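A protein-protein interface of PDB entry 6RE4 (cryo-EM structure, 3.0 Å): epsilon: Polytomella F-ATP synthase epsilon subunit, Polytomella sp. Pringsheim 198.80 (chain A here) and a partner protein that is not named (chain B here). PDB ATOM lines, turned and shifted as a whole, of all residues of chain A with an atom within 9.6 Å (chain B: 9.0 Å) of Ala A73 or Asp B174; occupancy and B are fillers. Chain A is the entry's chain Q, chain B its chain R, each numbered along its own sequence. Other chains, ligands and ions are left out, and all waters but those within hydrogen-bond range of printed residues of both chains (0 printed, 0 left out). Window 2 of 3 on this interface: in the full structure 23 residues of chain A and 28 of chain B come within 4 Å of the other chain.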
ATOM      1  N   VAL A  11      -8.645  17.669 -14.231  1.00  0.00           N
ATOM      2  CA  VAL A  11      -9.470  16.576 -14.734  1.00  0.00           C
ATOM      3  C   VAL A  11     -10.245  16.961 -15.977  1.00  0.00           C
ATOM      4  O   VAL A  11     -10.874  16.094 -16.593  1.00  0.00           O
ATOM      5  CB  VAL A  11     -10.484  16.080 -13.688  1.00  0.00           C
ATOM      6  CG1 VAL A  11      -9.783  15.711 -12.396  1.00  0.00           C
ATOM      7  CG2 VAL A  11     -11.547  17.131 -13.451  1.00  0.00           C
ATOM      8  N   ALA A  12     -10.228  18.236 -16.364  1.00  0.00           N
ATOM      9  CA  ALA A  12     -10.856  18.692 -17.592  1.00  0.00           C
ATOM     10  C   ALA A  12      -9.846  18.921 -18.702  1.00  0.00           C
ATOM     11  O   ALA A  12     -10.162  19.597 -19.684  1.00  0.00           O
ATOM     12  CB  ALA A  12     -11.649  19.971 -17.339  1.00  0.00           C
ATOM     13  N   GLY A  13      -8.636  18.384 -18.561  1.00  0.00           N
ATOM     14  CA  GLY A  13      -7.614  18.551 -19.574  1.00  0.00           C
ATOM     15  C   GLY A  13      -7.029  19.939 -19.669  1.00  0.00           C
ATOM     16  O   GLY A  13      -6.434  20.280 -20.693  1.00  0.00           O
ATOM     17  N   MET A  14      -7.169  20.748 -18.624  1.00  0.00           N
ATOM     18  CA  MET A  14      -6.725  22.134 -18.613  1.00  0.00           C
ATOM     19  C   MET A  14      -5.610  22.297 -17.595  1.00  0.00           C
ATOM     20  O   MET A  14      -5.776  21.938 -16.428  1.00  0.00           O
ATOM     21  CB  MET A  14      -7.896  23.053 -18.277  1.00  0.00           C
ATOM     22  CG  MET A  14      -7.541  24.481 -18.040  1.00  0.00           C
ATOM     23  SD  MET A  14      -8.963  25.377 -17.411  1.00  0.00           S
ATOM     24  CE  MET A  14     -10.179  24.992 -18.645  1.00  0.00           C
ATOM     25  N   ARG A  18      -3.363  27.865 -17.894  1.00  0.00           N
ATOM     26  CA  ARG A  18      -4.542  28.252 -18.653  1.00  0.00           C
ATOM     27  C   ARG A  18      -5.713  28.586 -17.748  1.00  0.00           C
ATOM     28  O   ARG A  18      -6.432  29.548 -18.020  1.00  0.00           O
ATOM     29  CB  ARG A  18      -4.940  27.156 -19.622  1.00  0.00           C
ATOM     30  CG  ARG A  18      -5.957  27.628 -20.615  1.00  0.00           C
ATOM     31  CD  ARG A  18      -6.160  26.598 -21.672  1.00  0.00           C
ATOM     32  NE  ARG A  18      -4.936  26.352 -22.415  1.00  0.00           N
ATOM     33  CZ  ARG A  18      -4.764  26.701 -23.678  1.00  0.00           C
ATOM     34  NH1 ARG A  18      -5.737  27.314 -24.331  1.00  0.00           N
ATOM     35  NH2 ARG A  18      -3.621  26.432 -24.283  1.00  0.00           N
ATOM     36  N   ILE A  22      -7.375  32.220 -17.517  1.00  0.00           N
ATOM     37  CA  ILE A  22      -8.807  32.430 -17.716  1.00  0.00           C
ATOM     38  C   ILE A  22      -9.377  33.277 -16.592  1.00  0.00           C
ATOM     39  O   ILE A  22     -10.120  34.235 -16.835  1.00  0.00           O
ATOM     40  CB  ILE A  22      -9.532  31.076 -17.833  1.00  0.00           C
ATOM     41  CG1 ILE A  22      -9.293  30.448 -19.195  1.00  0.00           C
ATOM     42  CG2 ILE A  22     -11.011  31.211 -17.589  1.00  0.00           C
ATOM     43  CD1 ILE A  22      -9.716  29.020 -19.252  1.00  0.00           C
ATOM     44  N   ILE A  69      -6.452  34.251 -23.364  1.00  0.00           N
ATOM     45  CA  ILE A  69      -6.000  32.899 -23.675  1.00  0.00           C
ATOM     46  C   ILE A  69      -7.218  32.183 -24.261  1.00  0.00           C
ATOM     47  O   ILE A  69      -8.351  32.625 -24.007  1.00  0.00           O
ATOM     48  CB  ILE A  69      -5.411  32.231 -22.412  1.00  0.00           C
ATOM     49  CG1 ILE A  69      -4.097  31.507 -22.725  1.00  0.00           C
ATOM     50  CG2 ILE A  69      -6.395  31.259 -21.769  1.00  0.00           C
ATOM     51  CD1 ILE A  69      -3.287  31.128 -21.527  1.00  0.00           C
ATOM     52  N   PRO A  70      -7.066  31.141 -25.085  1.00  0.00           N
ATOM     53  CA  PRO A  70      -8.251  30.474 -25.648  1.00  0.00           C
ATOM     54  C   PRO A  70      -9.013  29.697 -24.586  1.00  0.00           C
ATOM     55  O   PRO A  70      -8.475  28.780 -23.965  1.00  0.00           O
ATOM     56  CB  PRO A  70      -7.663  29.536 -26.707  1.00  0.00           C
ATOM     57  CG  PRO A  70      -6.327  30.052 -26.986  1.00  0.00           C
ATOM     58  CD  PRO A  70      -5.837  30.647 -25.724  1.00  0.00           C
ATOM     59  N   LYS A  71     -10.281  30.056 -24.391  1.00  0.00           N
ATOM     60  CA  LYS A  71     -11.116  29.301 -23.474  1.00  0.00           C
ATOM     61  C   LYS A  71     -11.538  27.959 -24.044  1.00  0.00           C
ATOM     62  O   LYS A  71     -11.981  27.096 -23.282  1.00  0.00           O
ATOM     63  CB  LYS A  71     -12.373  30.087 -23.101  1.00  0.00           C
ATOM     64  CG  LYS A  71     -12.121  31.446 -22.501  1.00  0.00           C
ATOM     65  CD  LYS A  71     -13.409  31.998 -21.925  1.00  0.00           C
ATOM     66  CE  LYS A  71     -13.321  33.484 -21.672  1.00  0.00           C
ATOM     67  NZ  LYS A  71     -13.191  34.243 -22.937  1.00  0.00           N
ATOM     68  N   THR A  72     -11.428  27.769 -25.354  1.00  0.00           N
ATOM     69  CA  THR A  72     -11.854  26.537 -25.994  1.00  0.00           C
ATOM     70  C   THR A  72     -10.712  25.528 -26.035  1.00  0.00           C
ATOM     71  O   THR A  72      -9.531  25.877 -26.049  1.00  0.00           O
ATOM     72  CB  THR A  72     -12.366  26.816 -27.402  1.00  0.00           C
ATOM     73  OG1 THR A  72     -11.256  26.908 -28.301  1.00  0.00           O
ATOM     74  CG2 THR A  72     -13.130  28.133 -27.425  1.00  0.00           C
ATOM     75  N   ALA A  73     -11.089  24.254 -26.090  1.00  0.00           N
ATOM     76  CA  ALA A  73     -10.146  23.168 -25.869  1.00  0.00           C
ATOM     77  C   ALA A  73      -9.230  22.979 -27.068  1.00  0.00           C
ATOM     78  O   ALA A  73      -9.684  22.960 -28.217  1.00  0.00           O
ATOM     79  CB  ALA A  73     -10.897  21.870 -25.586  1.00  0.00           C
ATOM     80  N   ASN A  74      -7.939  22.829 -26.792  1.00  0.00           N
ATOM     81  CA  ASN A  74      -6.949  22.617 -27.838  1.00  0.00           C
ATOM     82  C   ASN A  74      -5.955  21.546 -27.416  1.00  0.00           C
ATOM     83  O   ASN A  74      -6.012  21.047 -26.294  1.00  0.00           O
ATOM     84  CB  ASN A  74      -6.227  23.926 -28.154  1.00  0.00           C
ATOM     85  CG  ASN A  74      -7.119  24.916 -28.869  1.00  0.00           C
ATOM     86  OD1 ASN A  74      -7.810  24.568 -29.825  1.00  0.00           O
ATOM     87  ND2 ASN A  74      -7.136  26.152 -28.385  1.00  0.00           N
ATOM     88  N   ALA B 170     -24.939  29.314 -19.306  1.00  0.00           N
ATOM     89  CA  ALA B 170     -24.294  28.520 -20.344  1.00  0.00           C
ATOM     90  C   ALA B 170     -23.725  27.237 -19.750  1.00  0.00           C
ATOM     91  O   ALA B 170     -22.802  27.278 -18.934  1.00  0.00           O
ATOM     92  CB  ALA B 170     -23.206  29.335 -21.035  1.00  0.00           C
ATOM     93  N   GLN B 171     -24.283  26.096 -20.157  1.00  0.00           N
ATOM     94  CA  GLN B 171     -23.729  24.782 -19.845  1.00  0.00           C
ATOM     95  C   GLN B 171     -23.436  24.057 -21.154  1.00  0.00           C
ATOM     96  O   GLN B 171     -24.352  23.517 -21.790  1.00  0.00           O
ATOM     97  CB  GLN B 171     -24.681  23.960 -18.971  1.00  0.00           C
ATOM     98  CG  GLN B 171     -25.032  24.594 -17.638  1.00  0.00           C
ATOM     99  CD  GLN B 171     -26.495  24.421 -17.279  1.00  0.00           C
ATOM    100  OE1 GLN B 171     -27.222  23.676 -17.933  1.00  0.00           O
ATOM    101  NE2 GLN B 171     -26.930  25.102 -16.228  1.00  0.00           N
ATOM    102  N   PRO B 172     -22.185  24.011 -21.596  1.00  0.00           N
ATOM    103  CA  PRO B 172     -21.861  23.413 -22.893  1.00  0.00           C
ATOM    104  C   PRO B 172     -21.792  21.890 -22.831  1.00  0.00           C
ATOM    105  O   PRO B 172     -22.035  21.263 -21.802  1.00  0.00           O
ATOM    106  CB  PRO B 172     -20.495  24.015 -23.216  1.00  0.00           C
ATOM    107  CG  PRO B 172     -19.891  24.269 -21.887  1.00  0.00           C
ATOM    108  CD  PRO B 172     -21.019  24.672 -20.987  1.00  0.00           C
ATOM    109  N   THR B 173     -21.439  21.306 -23.977  1.00  0.00           N
ATOM    110  CA  THR B 173     -21.325  19.867 -24.165  1.00  0.00           C
ATOM    111  C   THR B 173     -19.935  19.353 -23.802  1.00  0.00           C
ATOM    112  O   THR B 173     -19.782  18.174 -23.460  1.00  0.00           O
ATOM    113  CB  THR B 173     -21.668  19.524 -25.630  1.00  0.00           C
ATOM    114  OG1 THR B 173     -22.885  20.188 -25.991  1.00  0.00           O
ATOM    115  CG2 THR B 173     -21.898  18.030 -25.844  1.00  0.00           C
ATOM    116  N   ASP B 174     -18.936  20.229 -23.800  1.00  0.00           N
ATOM    117  CA  ASP B 174     -17.558  19.867 -23.527  1.00  0.00           C
ATOM    118  C   ASP B 174     -17.213  20.187 -22.079  1.00  0.00           C
ATOM    119  O   ASP B 174     -17.767  21.113 -21.479  1.00  0.00           O
ATOM    120  CB  ASP B 174     -16.614  20.607 -24.479  1.00  0.00           C
ATOM    121  CG  ASP B 174     -15.230  20.012 -24.510  1.00  0.00           C
ATOM    122  OD1 ASP B 174     -14.254  20.780 -24.609  1.00  0.00           O
ATOM    123  OD2 ASP B 174     -15.119  18.773 -24.446  1.00  0.00           O
ATOM    124  N   GLU B 175     -16.296  19.395 -21.518  1.00  0.00           N
ATOM    125  CA  GLU B 175     -15.865  19.578 -20.137  1.00  0.00           C
ATOM    126  C   GLU B 175     -14.917  20.758 -19.974  1.00  0.00           C
ATOM    127  O   GLU B 175     -14.762  21.265 -18.860  1.00  0.00           O
ATOM    128  CB  GLU B 175     -15.192  18.298 -19.631  1.00  0.00           C
ATOM    129  CG  GLU B 175     -13.815  18.033 -20.239  1.00  0.00           C
ATOM    130  CD  GLU B 175     -13.862  17.277 -21.554  1.00  0.00           C
ATOM    131  OE1 GLU B 175     -14.959  17.120 -22.124  1.00  0.00           O
ATOM    132  OE2 GLU B 175     -12.790  16.852 -22.029  1.00  0.00           O
ATOM    133  N   PHE B 176     -14.289  21.207 -21.058  1.00  0.00           N
ATOM    134  CA  PHE B 176     -13.290  22.261 -20.971  1.00  0.00           C
ATOM    135  C   PHE B 176     -13.941  23.605 -20.689  1.00  0.00           C
ATOM    136  O   PHE B 176     -13.581  24.302 -19.731  1.00  0.00           O
ATOM    137  CB  PHE B 176     -12.503  22.304 -22.273  1.00  0.00           C
ATOM    138  CG  PHE B 176     -11.150  22.906 -22.148  1.00  0.00           C
ATOM    139  CD1 PHE B 176     -10.053  22.116 -21.863  1.00  0.00           C
ATOM    140  CD2 PHE B 176     -10.970  24.260 -22.339  1.00  0.00           C
ATOM    141  CE1 PHE B 176      -8.800  22.669 -21.763  1.00  0.00           C
ATOM    142  CE2 PHE B 176      -9.724  24.823 -22.240  1.00  0.00           C
ATOM    143  CZ  PHE B 176      -8.634  24.025 -21.950  1.00  0.00           C
ATOM    144  N   GLU B 177     -14.927  23.977 -21.500  1.00  0.00           N
ATOM    145  CA  GLU B 177     -15.681  25.188 -21.217  1.00  0.00           C
ATOM    146  C   GLU B 177     -16.587  25.014 -20.002  1.00  0.00           C
ATOM    147  O   GLU B 177     -16.992  26.008 -19.398  1.00  0.00           O
ATOM    148  CB  GLU B 177     -16.475  25.596 -22.452  1.00  0.00           C
ATOM    149  CG  GLU B 177     -15.600  25.974 -23.636  1.00  0.00           C
ATOM    150  CD  GLU B 177     -15.356  24.826 -24.599  1.00  0.00           C
ATOM    151  OE1 GLU B 177     -15.160  25.092 -25.804  1.00  0.00           O
ATOM    152  OE2 GLU B 177     -15.350  23.662 -24.157  1.00  0.00           O
ATOM    153  N   GLN B 178     -16.882  23.771 -19.610  1.00  0.00           N
ATOM    154  CA  GLN B 178     -17.540  23.518 -18.333  1.00  0.00           C
ATOM    155  C   GLN B 178     -16.656  23.947 -17.167  1.00  0.00           C
ATOM    156  O   GLN B 178     -17.114  24.625 -16.241  1.00  0.00           O
ATOM    157  CB  GLN B 178     -17.898  22.034 -18.225  1.00  0.00           C
ATOM    158  CG  GLN B 178     -18.116  21.518 -16.814  1.00  0.00           C
ATOM    159  CD  GLN B 178     -19.352  22.092 -16.168  1.00  0.00           C
ATOM    160  OE1 GLN B 178     -20.471  21.758 -16.546  1.00  0.00           O
ATOM    161  NE2 GLN B 178     -19.157  22.966 -15.188  1.00  0.00           N
ATOM    162  N   ALA B 179     -15.375  23.567 -17.208  1.00  0.00           N
ATOM    163  CA  ALA B 179     -14.432  23.997 -16.181  1.00  0.00           C
ATOM    164  C   ALA B 179     -14.212  25.499 -16.230  1.00  0.00           C
ATOM    165  O   ALA B 179     -14.071  26.146 -15.187  1.00  0.00           O
ATOM    166  CB  ALA B 179     -13.102  23.266 -16.347  1.00  0.00           C
ATOM    167  N   ALA B 180     -14.201  26.070 -17.436  1.00  0.00           N
ATOM    168  CA  ALA B 180     -14.070  27.518 -17.567  1.00  0.00           C
ATOM    169  C   ALA B 180     -15.277  28.242 -16.981  1.00  0.00           C
ATOM    170  O   ALA B 180     -15.126  29.274 -16.326  1.00  0.00           O
ATOM    171  CB  ALA B 180     -13.871  27.894 -19.030  1.00  0.00           C
ATOM    172  N   ASN B 181     -16.475  27.687 -17.159  1.00  0.00           N
ATOM    173  CA  ASN B 181     -17.674  28.317 -16.622  1.00  0.00           C
ATOM    174  C   ASN B 181     -17.758  28.148 -15.114  1.00  0.00           C
ATOM    175  O   ASN B 181     -18.283  29.019 -14.414  1.00  0.00           O
ATOM    176  CB  ASN B 181     -18.914  27.730 -17.285  1.00  0.00           C
ATOM    177  CG  ASN B 181     -20.033  28.732 -17.401  1.00  0.00           C
ATOM    178  OD1 ASN B 181     -19.816  29.871 -17.813  1.00  0.00           O
ATOM    179  ND2 ASN B 181     -21.242  28.317 -17.044  1.00  0.00           N
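The backbone carbonyl oxygen (O) of Pro A70 is in hydrogen-bond range of the guanidinium group (NH1) of Arg A18, 3.1 Å away.
The side-chain amide nitrogen (ND2) of Asn A74 sits at hydrogen-bond distance from the backbone carbonyl oxygen (O) of Thr A72.
Ala A12 touches Glu B175 (CB to O, 3.7 Å).
Phe B176 touches Ala A12 (CD1 to O, 3.3 Å).
CB of Ala A12 touches CB of Ala B179, 3.7 Å away.
O of Gly A13 touches CE1 of Phe B176 (3.5 Å).
Met A14 touches Phe B176.
Arg A18 touches Phe B176 (CD to CZ, 3.6 Å).
CD2 of Phe B176 touches O of Lys A71, at 3.2 Å.
Lys A71 touches Glu B177 (O to CG, 3.8 Å).
C of Thr A72 touches CD2 of Phe B176, 3.9 Å away.
Thr A72 touches Glu B177 (CA to OE1, 3.6 Å).
Of the printed residues of chain B, Ala A12 touches Glu B175 (3.7 Å), Phe B176 (3.3 Å) and Ala B179 (3.7 Å).
Of the printed residues of chain B, Arg A18 touches Phe B176 (3.6 Å).
Of the printed residues of chain B, Lys A71 touches Phe B176 (3.2 Å) and Glu B177 (3.8 Å).
Thr A72 touches just these residues of chain B: Phe B176 (3.9 Å) and Glu B177 (3.6 Å).
Of chain B, only Asp B174 and Phe B176 come within 4 Å of Ala A73.
No residue of chain B comes within 4 Å of Asn A74.
Thr B173 touches none of the printed residues of chain A.
Asp B174 touches one residue of chain A.
Of the printed residues of chain A, Ala B179 touches Ala A12.
The nearest residue of chain B that does not touch Ala A73 is Glu B177 (4.2 Å).
The nearest residue of chain A that does not touch Asp B174 is Thr A72 (6.1 Å).
The nearest printed residue of chain B that does not touch Gly A13 is Glu B175 (5.5 Å).
Hydrophobic or aromatic side chains of chain A within 4 Å of the printed part of chain B: Ala A12, Met A14 and Ala A73.
Hydrophobic or aromatic side chains of chain B that line the printed part of chain A: Phe B176 and Ala B179.
Along chain B the printed residues that touch a printed residue of chain A span positions 174 to 179.
Among the printed residues, 12 pairs touch across the chains.
Among the printed residues, no Asp or Glu carboxylate lies within 4 Å of a Lys or Arg side-chain nitrogen of the other chain.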
